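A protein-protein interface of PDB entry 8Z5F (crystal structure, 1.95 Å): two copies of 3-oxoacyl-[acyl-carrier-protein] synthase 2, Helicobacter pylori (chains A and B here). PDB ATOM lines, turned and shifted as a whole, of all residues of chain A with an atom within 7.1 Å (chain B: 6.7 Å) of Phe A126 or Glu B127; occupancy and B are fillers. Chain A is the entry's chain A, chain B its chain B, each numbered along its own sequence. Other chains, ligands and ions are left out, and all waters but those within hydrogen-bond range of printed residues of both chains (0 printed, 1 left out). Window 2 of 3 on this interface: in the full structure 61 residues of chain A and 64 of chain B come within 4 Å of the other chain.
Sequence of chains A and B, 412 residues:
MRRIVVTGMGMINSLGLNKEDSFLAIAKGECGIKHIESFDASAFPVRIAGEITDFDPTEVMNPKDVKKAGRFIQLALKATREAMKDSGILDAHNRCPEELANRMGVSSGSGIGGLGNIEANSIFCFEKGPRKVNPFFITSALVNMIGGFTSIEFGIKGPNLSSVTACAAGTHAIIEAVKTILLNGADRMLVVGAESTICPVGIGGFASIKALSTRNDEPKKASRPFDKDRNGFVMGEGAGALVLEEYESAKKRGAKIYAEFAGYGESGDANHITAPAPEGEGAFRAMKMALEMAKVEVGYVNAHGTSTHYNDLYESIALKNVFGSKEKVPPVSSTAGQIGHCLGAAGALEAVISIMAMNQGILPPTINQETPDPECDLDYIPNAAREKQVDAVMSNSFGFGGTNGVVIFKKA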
ATOM      1  N   ALA A 120      -7.834  14.593 -13.114  1.00  0.00           N
ATOM      2  CA  ALA A 120      -8.599  13.417 -13.538  1.00  0.00           C
ATOM      3  C   ALA A 120      -9.368  13.689 -14.829  1.00  0.00           C
ATOM      4  O   ALA A 120      -9.374  12.859 -15.748  1.00  0.00           O
ATOM      5  CB  ALA A 120      -9.555  12.965 -12.430  1.00  0.00           C
ATOM      6  N   ASN A 121     -10.023  14.845 -14.928  1.00  0.00           N
ATOM      7  CA  ASN A 121     -10.782  15.116 -16.143  1.00  0.00           C
ATOM      8  C   ASN A 121      -9.887  15.478 -17.314  1.00  0.00           C
ATOM      9  O   ASN A 121     -10.274  15.242 -18.464  1.00  0.00           O
ATOM     10  CB  ASN A 121     -11.805  16.215 -15.905  1.00  0.00           C
ATOM     11  CG  ASN A 121     -13.018  15.704 -15.158  1.00  0.00           C
ATOM     12  OD1 ASN A 121     -14.009  15.307 -15.768  1.00  0.00           O
ATOM     13  ND2 ASN A 121     -12.931  15.674 -13.828  1.00  0.00           N
ATOM     14  N   SER A 122      -8.706  16.063 -17.062  1.00  0.00           N
ATOM     15  CA  SER A 122      -7.758  16.279 -18.150  1.00  0.00           C
ATOM     16  C   SER A 122      -7.377  14.961 -18.800  1.00  0.00           C
ATOM     17  O   SER A 122      -7.269  14.871 -20.027  1.00  0.00           O
ATOM     18  CB  SER A 122      -6.502  16.980 -17.639  1.00  0.00           C
ATOM     19  OG  SER A 122      -6.804  18.268 -17.140  1.00  0.00           O
ATOM     20  N   ILE A 123      -7.198  13.923 -17.982  1.00  0.00           N
ATOM     21  CA  ILE A 123      -6.797  12.614 -18.475  1.00  0.00           C
ATOM     22  C   ILE A 123      -7.966  11.905 -19.166  1.00  0.00           C
ATOM     23  O   ILE A 123      -7.786  11.304 -20.231  1.00  0.00           O
ATOM     24  CB  ILE A 123      -6.210  11.791 -17.308  1.00  0.00           C
ATOM     25  CG1 ILE A 123      -4.858  12.364 -16.880  1.00  0.00           C
ATOM     26  CG2 ILE A 123      -6.070  10.322 -17.669  1.00  0.00           C
ATOM     27  CD1 ILE A 123      -4.491  12.039 -15.453  1.00  0.00           C
ATOM     28  N   PHE A 124      -9.171  11.957 -18.578  1.00  0.00           N
ATOM     29  CA  PHE A 124     -10.367  11.467 -19.271  1.00  0.00           C
ATOM     30  C   PHE A 124     -10.446  12.031 -20.682  1.00  0.00           C
ATOM     31  O   PHE A 124     -10.667  11.299 -21.652  1.00  0.00           O
ATOM     32  CB  PHE A 124     -11.654  11.865 -18.542  1.00  0.00           C
ATOM     33  CG  PHE A 124     -11.839  11.245 -17.193  1.00  0.00           C
ATOM     34  CD1 PHE A 124     -11.196  10.075 -16.844  1.00  0.00           C
ATOM     35  CD2 PHE A 124     -12.681  11.860 -16.256  1.00  0.00           C
ATOM     36  CE1 PHE A 124     -11.377   9.519 -15.577  1.00  0.00           C
ATOM     37  CE2 PHE A 124     -12.863  11.317 -14.978  1.00  0.00           C
ATOM     38  CZ  PHE A 124     -12.210  10.138 -14.645  1.00  0.00           C
ATOM     39  N   CYS A 125     -10.329  13.354 -20.803  1.00  0.00           N
ATOM     40  CA  CYS A 125     -10.479  13.982 -22.108  1.00  0.00           C
ATOM     41  C   CYS A 125      -9.393  13.511 -23.063  1.00  0.00           C
ATOM     42  O   CYS A 125      -9.661  13.228 -24.234  1.00  0.00           O
ATOM     43  CB  CYS A 125     -10.452  15.504 -21.956  1.00  0.00           C
ATOM     44  SG  CYS A 125     -11.073  16.407 -23.391  1.00  0.00           S
ATOM     45  N   PHE A 126      -8.165  13.393 -22.569  1.00  0.00           N
ATOM     46  CA  PHE A 126      -7.048  13.003 -23.416  1.00  0.00           C
ATOM     47  C   PHE A 126      -7.174  11.550 -23.874  1.00  0.00           C
ATOM     48  O   PHE A 126      -6.838  11.227 -25.017  1.00  0.00           O
ATOM     49  CB  PHE A 126      -5.752  13.239 -22.643  1.00  0.00           C
ATOM     50  CG  PHE A 126      -4.502  12.782 -23.350  1.00  0.00           C
ATOM     51  CD1 PHE A 126      -3.868  13.604 -24.271  1.00  0.00           C
ATOM     52  CD2 PHE A 126      -3.930  11.550 -23.049  1.00  0.00           C
ATOM     53  CE1 PHE A 126      -2.693  13.197 -24.904  1.00  0.00           C
ATOM     54  CE2 PHE A 126      -2.754  11.137 -23.669  1.00  0.00           C
ATOM     55  CZ  PHE A 126      -2.133  11.963 -24.599  1.00  0.00           C
ATOM     56  N   GLU A 127      -7.662  10.664 -23.002  1.00  0.00           N
ATOM     57  CA  GLU A 127      -7.655   9.235 -23.297  1.00  0.00           C
ATOM     58  C   GLU A 127      -8.862   8.819 -24.128  1.00  0.00           C
ATOM     59  O   GLU A 127      -8.743   7.957 -25.003  1.00  0.00           O
ATOM     60  CB  GLU A 127      -7.606   8.418 -21.997  1.00  0.00           C
ATOM     61  CG  GLU A 127      -6.207   7.891 -21.622  1.00  0.00           C
ATOM     62  CD  GLU A 127      -6.230   6.510 -20.942  1.00  0.00           C
ATOM     63  OE1 GLU A 127      -6.892   6.370 -19.886  1.00  0.00           O
ATOM     64  OE2 GLU A 127      -5.573   5.568 -21.454  1.00  0.00           O
ATOM     65  N   LYS A 128     -10.024   9.415 -23.781  1.00  0.00           N
ATOM     66  CA  LYS A 128     -11.293   8.959 -24.400  1.00  0.00           C
ATOM     67  C   LYS A 128     -12.172  10.083 -24.935  1.00  0.00           C
ATOM     68  O   LYS A 128     -13.309   9.765 -25.296  1.00  0.00           O
ATOM     69  CB  LYS A 128     -12.094   8.163 -23.371  1.00  0.00           C
ATOM     70  CG  LYS A 128     -11.640   8.385 -21.938  1.00  0.00           C
ATOM     71  CD  LYS A 128     -10.751   7.302 -21.385  1.00  0.00           C
ATOM     72  CE  LYS A 128     -10.816   7.262 -19.876  1.00  0.00           C
ATOM     73  NZ  LYS A 128     -12.130   7.744 -19.387  1.00  0.00           N
ATOM     74  N   GLY A 129     -11.666  11.310 -25.051  1.00  0.00           N
ATOM     75  CA  GLY A 129     -12.407  12.402 -25.643  1.00  0.00           C
ATOM     76  C   GLY A 129     -13.294  13.196 -24.694  1.00  0.00           C
ATOM     77  O   GLY A 129     -13.582  12.789 -23.560  1.00  0.00           O
ATOM     78  N   PRO A 130     -13.778  14.346 -25.176  1.00  0.00           N
ATOM     79  CA  PRO A 130     -14.547  15.251 -24.305  1.00  0.00           C
ATOM     80  C   PRO A 130     -15.854  14.667 -23.809  1.00  0.00           C
ATOM     81  O   PRO A 130     -16.425  15.205 -22.856  1.00  0.00           O
ATOM     82  CB  PRO A 130     -14.788  16.477 -25.199  1.00  0.00           C
ATOM     83  CG  PRO A 130     -14.692  15.934 -26.615  1.00  0.00           C
ATOM     84  CD  PRO A 130     -13.656  14.859 -26.553  1.00  0.00           C
ATOM     85  N   VAL A 133     -15.592  13.788 -20.162  1.00  0.00           N
ATOM     86  CA  VAL A 133     -15.492  14.815 -19.132  1.00  0.00           C
ATOM     87  C   VAL A 133     -16.739  14.772 -18.265  1.00  0.00           C
ATOM     88  O   VAL A 133     -17.872  14.849 -18.764  1.00  0.00           O
ATOM     89  CB  VAL A 133     -15.300  16.208 -19.748  1.00  0.00           C
ATOM     90  CG1 VAL A 133     -15.391  17.284 -18.648  1.00  0.00           C
ATOM     91  CG2 VAL A 133     -13.966  16.298 -20.514  1.00  0.00           C
ATOM     92  N   GLU B 119      -3.560  20.913 -17.357  1.00  0.00           N
ATOM     93  CA  GLU B 119      -3.944  19.789 -18.195  1.00  0.00           C
ATOM     94  C   GLU B 119      -2.718  19.104 -18.786  1.00  0.00           C
ATOM     95  O   GLU B 119      -2.583  17.876 -18.710  1.00  0.00           O
ATOM     96  CB  GLU B 119      -4.886  20.304 -19.280  1.00  0.00           C
ATOM     97  CG  GLU B 119      -5.047  19.450 -20.517  1.00  0.00           C
ATOM     98  CD  GLU B 119      -6.034  20.100 -21.489  1.00  0.00           C
ATOM     99  OE1 GLU B 119      -5.746  21.219 -21.985  1.00  0.00           O
ATOM    100  OE2 GLU B 119      -7.101  19.502 -21.738  1.00  0.00           O
ATOM    101  N   SER B 122      -0.700  17.335 -16.097  1.00  0.00           N
ATOM    102  CA  SER B 122      -1.446  16.174 -15.615  1.00  0.00           C
ATOM    103  C   SER B 122      -1.238  14.978 -16.531  1.00  0.00           C
ATOM    104  O   SER B 122      -1.072  13.838 -16.064  1.00  0.00           O
ATOM    105  CB  SER B 122      -2.930  16.518 -15.504  1.00  0.00           C
ATOM    106  OG  SER B 122      -3.118  17.548 -14.535  1.00  0.00           O
ATOM    107  N   ILE B 123      -1.233  15.230 -17.844  1.00  0.00           N
ATOM    108  CA  ILE B 123      -1.018  14.187 -18.834  1.00  0.00           C
ATOM    109  C   ILE B 123       0.438  13.731 -18.834  1.00  0.00           C
ATOM    110  O   ILE B 123       0.712  12.528 -18.891  1.00  0.00           O
ATOM    111  CB  ILE B 123      -1.469  14.690 -20.218  1.00  0.00           C
ATOM    112  CG1 ILE B 123      -2.999  14.805 -20.259  1.00  0.00           C
ATOM    113  CG2 ILE B 123      -0.975  13.777 -21.320  1.00  0.00           C
ATOM    114  CD1 ILE B 123      -3.496  15.843 -21.216  1.00  0.00           C
ATOM    115  N   PHE B 124       1.366  14.677 -18.729  1.00  0.00           N
ATOM    116  CA  PHE B 124       2.796  14.296 -18.626  1.00  0.00           C
ATOM    117  C   PHE B 124       2.965  13.335 -17.446  1.00  0.00           C
ATOM    118  O   PHE B 124       3.610  12.285 -17.602  1.00  0.00           O
ATOM    119  CB  PHE B 124       3.672  15.534 -18.438  1.00  0.00           C
ATOM    120  CG  PHE B 124       3.614  16.547 -19.552  1.00  0.00           C
ATOM    121  CD1 PHE B 124       2.935  16.277 -20.729  1.00  0.00           C
ATOM    122  CD2 PHE B 124       4.222  17.784 -19.412  1.00  0.00           C
ATOM    123  CE1 PHE B 124       2.879  17.215 -21.747  1.00  0.00           C
ATOM    124  CE2 PHE B 124       4.164  18.722 -20.430  1.00  0.00           C
ATOM    125  CZ  PHE B 124       3.494  18.436 -21.596  1.00  0.00           C
ATOM    126  N   CYS B 125       2.395  13.692 -16.294  1.00  0.00           N
ATOM    127  CA  CYS B 125       2.532  12.853 -15.115  1.00  0.00           C
ATOM    128  C   CYS B 125       1.774  11.545 -15.288  1.00  0.00           C
ATOM    129  O   CYS B 125       2.182  10.521 -14.736  1.00  0.00           O
ATOM    130  CB  CYS B 125       2.048  13.609 -13.872  1.00  0.00           C
ATOM    131  SG  CYS B 125       2.613  12.899 -12.279  1.00  0.00           S
ATOM    132  N   PHE B 126       0.685  11.554 -16.056  1.00  0.00           N
ATOM    133  CA  PHE B 126      -0.032  10.331 -16.375  1.00  0.00           C
ATOM    134  C   PHE B 126       0.553   9.593 -17.592  1.00  0.00           C
ATOM    135  O   PHE B 126      -0.036   8.628 -18.072  1.00  0.00           O
ATOM    136  CB  PHE B 126      -1.520  10.618 -16.598  1.00  0.00           C
ATOM    137  CG  PHE B 126      -2.318   9.412 -17.021  1.00  0.00           C
ATOM    138  CD1 PHE B 126      -2.664   8.447 -16.099  1.00  0.00           C
ATOM    139  CD2 PHE B 126      -2.683   9.227 -18.362  1.00  0.00           C
ATOM    140  CE1 PHE B 126      -3.368   7.332 -16.485  1.00  0.00           C
ATOM    141  CE2 PHE B 126      -3.384   8.100 -18.752  1.00  0.00           C
ATOM    142  CZ  PHE B 126      -3.729   7.157 -17.809  1.00  0.00           C
ATOM    143  N   GLU B 127       1.720   9.943 -18.076  1.00  0.00           N
ATOM    144  CA  GLU B 127       2.199   9.072 -19.139  1.00  0.00           C
ATOM    145  C   GLU B 127       3.620   8.637 -18.860  1.00  0.00           C
ATOM    146  O   GLU B 127       3.983   7.489 -19.136  1.00  0.00           O
ATOM    147  CB  GLU B 127       2.092   9.748 -20.505  1.00  0.00           C
ATOM    148  CG  GLU B 127       0.653   9.975 -20.940  1.00  0.00           C
ATOM    149  CD  GLU B 127       0.491   9.938 -22.446  1.00  0.00           C
ATOM    150  OE1 GLU B 127       1.185  10.725 -23.143  1.00  0.00           O
ATOM    151  OE2 GLU B 127      -0.321   9.111 -22.929  1.00  0.00           O
ATOM    152  N   LYS B 128       4.411   9.534 -18.289  1.00  0.00           N
ATOM    153  CA  LYS B 128       5.828   9.306 -18.098  1.00  0.00           C
ATOM    154  C   LYS B 128       6.258   9.408 -16.643  1.00  0.00           C
ATOM    155  O   LYS B 128       7.457   9.307 -16.365  1.00  0.00           O
ATOM    156  CB  LYS B 128       6.638  10.296 -18.953  1.00  0.00           C
ATOM    157  CG  LYS B 128       7.205   9.690 -20.255  1.00  0.00           C
ATOM    158  CD  LYS B 128       7.779   8.270 -20.039  1.00  0.00           C
ATOM    159  CE  LYS B 128       8.158   7.571 -21.364  1.00  0.00           C
ATOM    160  NZ  LYS B 128       9.584   7.095 -21.440  1.00  0.00           N
ATOM    161  N   GLY B 129       5.328   9.609 -15.711  1.00  0.00           N
ATOM    162  CA  GLY B 129       5.666   9.710 -14.309  1.00  0.00           C
ATOM    163  C   GLY B 129       5.934  11.132 -13.850  1.00  0.00           C
ATOM    164  O   GLY B 129       6.015  12.067 -14.650  1.00  0.00           O
ATOM    165  N   LYS B 132       8.437  13.915 -15.231  1.00  0.00           N
ATOM    166  CA  LYS B 132       8.143  14.633 -16.454  1.00  0.00           C
ATOM    167  C   LYS B 132       7.324  15.891 -16.224  1.00  0.00           C
ATOM    168  O   LYS B 132       6.936  16.541 -17.194  1.00  0.00           O
ATOM    169  CB  LYS B 132       7.437  13.705 -17.448  1.00  0.00           C
ATOM    170  CG  LYS B 132       7.888  13.914 -18.891  1.00  0.00           C
ATOM    171  CD  LYS B 132       9.427  13.977 -19.029  1.00  0.00           C
ATOM    172  CE  LYS B 132      10.167  12.810 -18.340  1.00  0.00           C
ATOM    173  NZ  LYS B 132      11.633  12.852 -18.599  1.00  0.00           N
ATOM    174  N   PRO B 200      -8.652  21.642 -24.571  1.00  0.00           N
ATOM    175  CA  PRO B 200      -9.612  20.520 -24.597  1.00  0.00           C
ATOM    176  C   PRO B 200     -10.430  20.391 -23.321  1.00  0.00           C
ATOM    177  O   PRO B 200     -11.670  20.378 -23.384  1.00  0.00           O
ATOM    178  CB  PRO B 200      -8.716  19.299 -24.854  1.00  0.00           C
ATOM    179  CG  PRO B 200      -7.536  19.849 -25.574  1.00  0.00           C
ATOM    180  CD  PRO B 200      -7.296  21.206 -24.971  1.00  0.00           C
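Ile A123 touches Ser B122, but with the chains exchanged Ser A122 does not touch Ile B123 (4.1 Å). Ile A123 touches Phe B126, and with the chains exchanged Phe A126 touches Ile B123. Phe A126 touches Glu B127, and with the chains exchanged Glu A127 touches Phe B126. 8 positions are printed for both chains. Of the 6 pairs that touch across the chains among the printed residues, 4 have their exchanged pair printed and touching as well.
Hydrophobic or aromatic side chains of chain B that line the printed part of chain A: Ile B123 and Phe B126. Of the 12 printed residues of chain A, 4 touch a printed residue of chain B. Printed residues of chain A that touch a printed residue of chain B: Ser A122, Ile A123, Phe A126 and Glu A127. Hydrophobic or aromatic side chains of chain A within 4 Å of the printed part of chain B: Ile A123 and Phe A126. Among the printed residues, 6 pairs touch across the chains. Among the printed residues, no Asp or Glu carboxylate lies within 4 Å of a Lys or Arg side-chain nitrogen of the other chain.
Among the printed residues, pairs that only touch across the chains: Phe A126 with Glu B127 (3.3 Å), Ser A122 with Glu B119 (3.4 Å), Ile A123 with Phe B126 (3.5 Å), Phe A126 with Ile B123 (3.7 Å), Glu A127 with Phe B126 (3.9 Å) and Ile A123 with Ser B122 (3.9 Å).
Of the printed residues of chain B, Ser A122 touches Glu B119 (3.4 Å). Of the printed residues of chain B, Ile A123 touches Ser B122 (3.9 Å) and Phe B126 (3.5 Å). Of chain B, only Ile B123 (3.7 Å) and Glu B127 (3.3 Å) come within 4 Å of Phe A126. Phe B124 touches none of the printed residues of chain A. Printed residues of chain A within 4 Å of Phe B126: Ile A123 (3.5 Å) and Glu A127 (3.9 Å). Of chain A, only Phe A126 comes within 4 Å of Glu B127. The nearest residue of chain A that does not touch Glu B127 is Glu A127 (6.2 Å).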
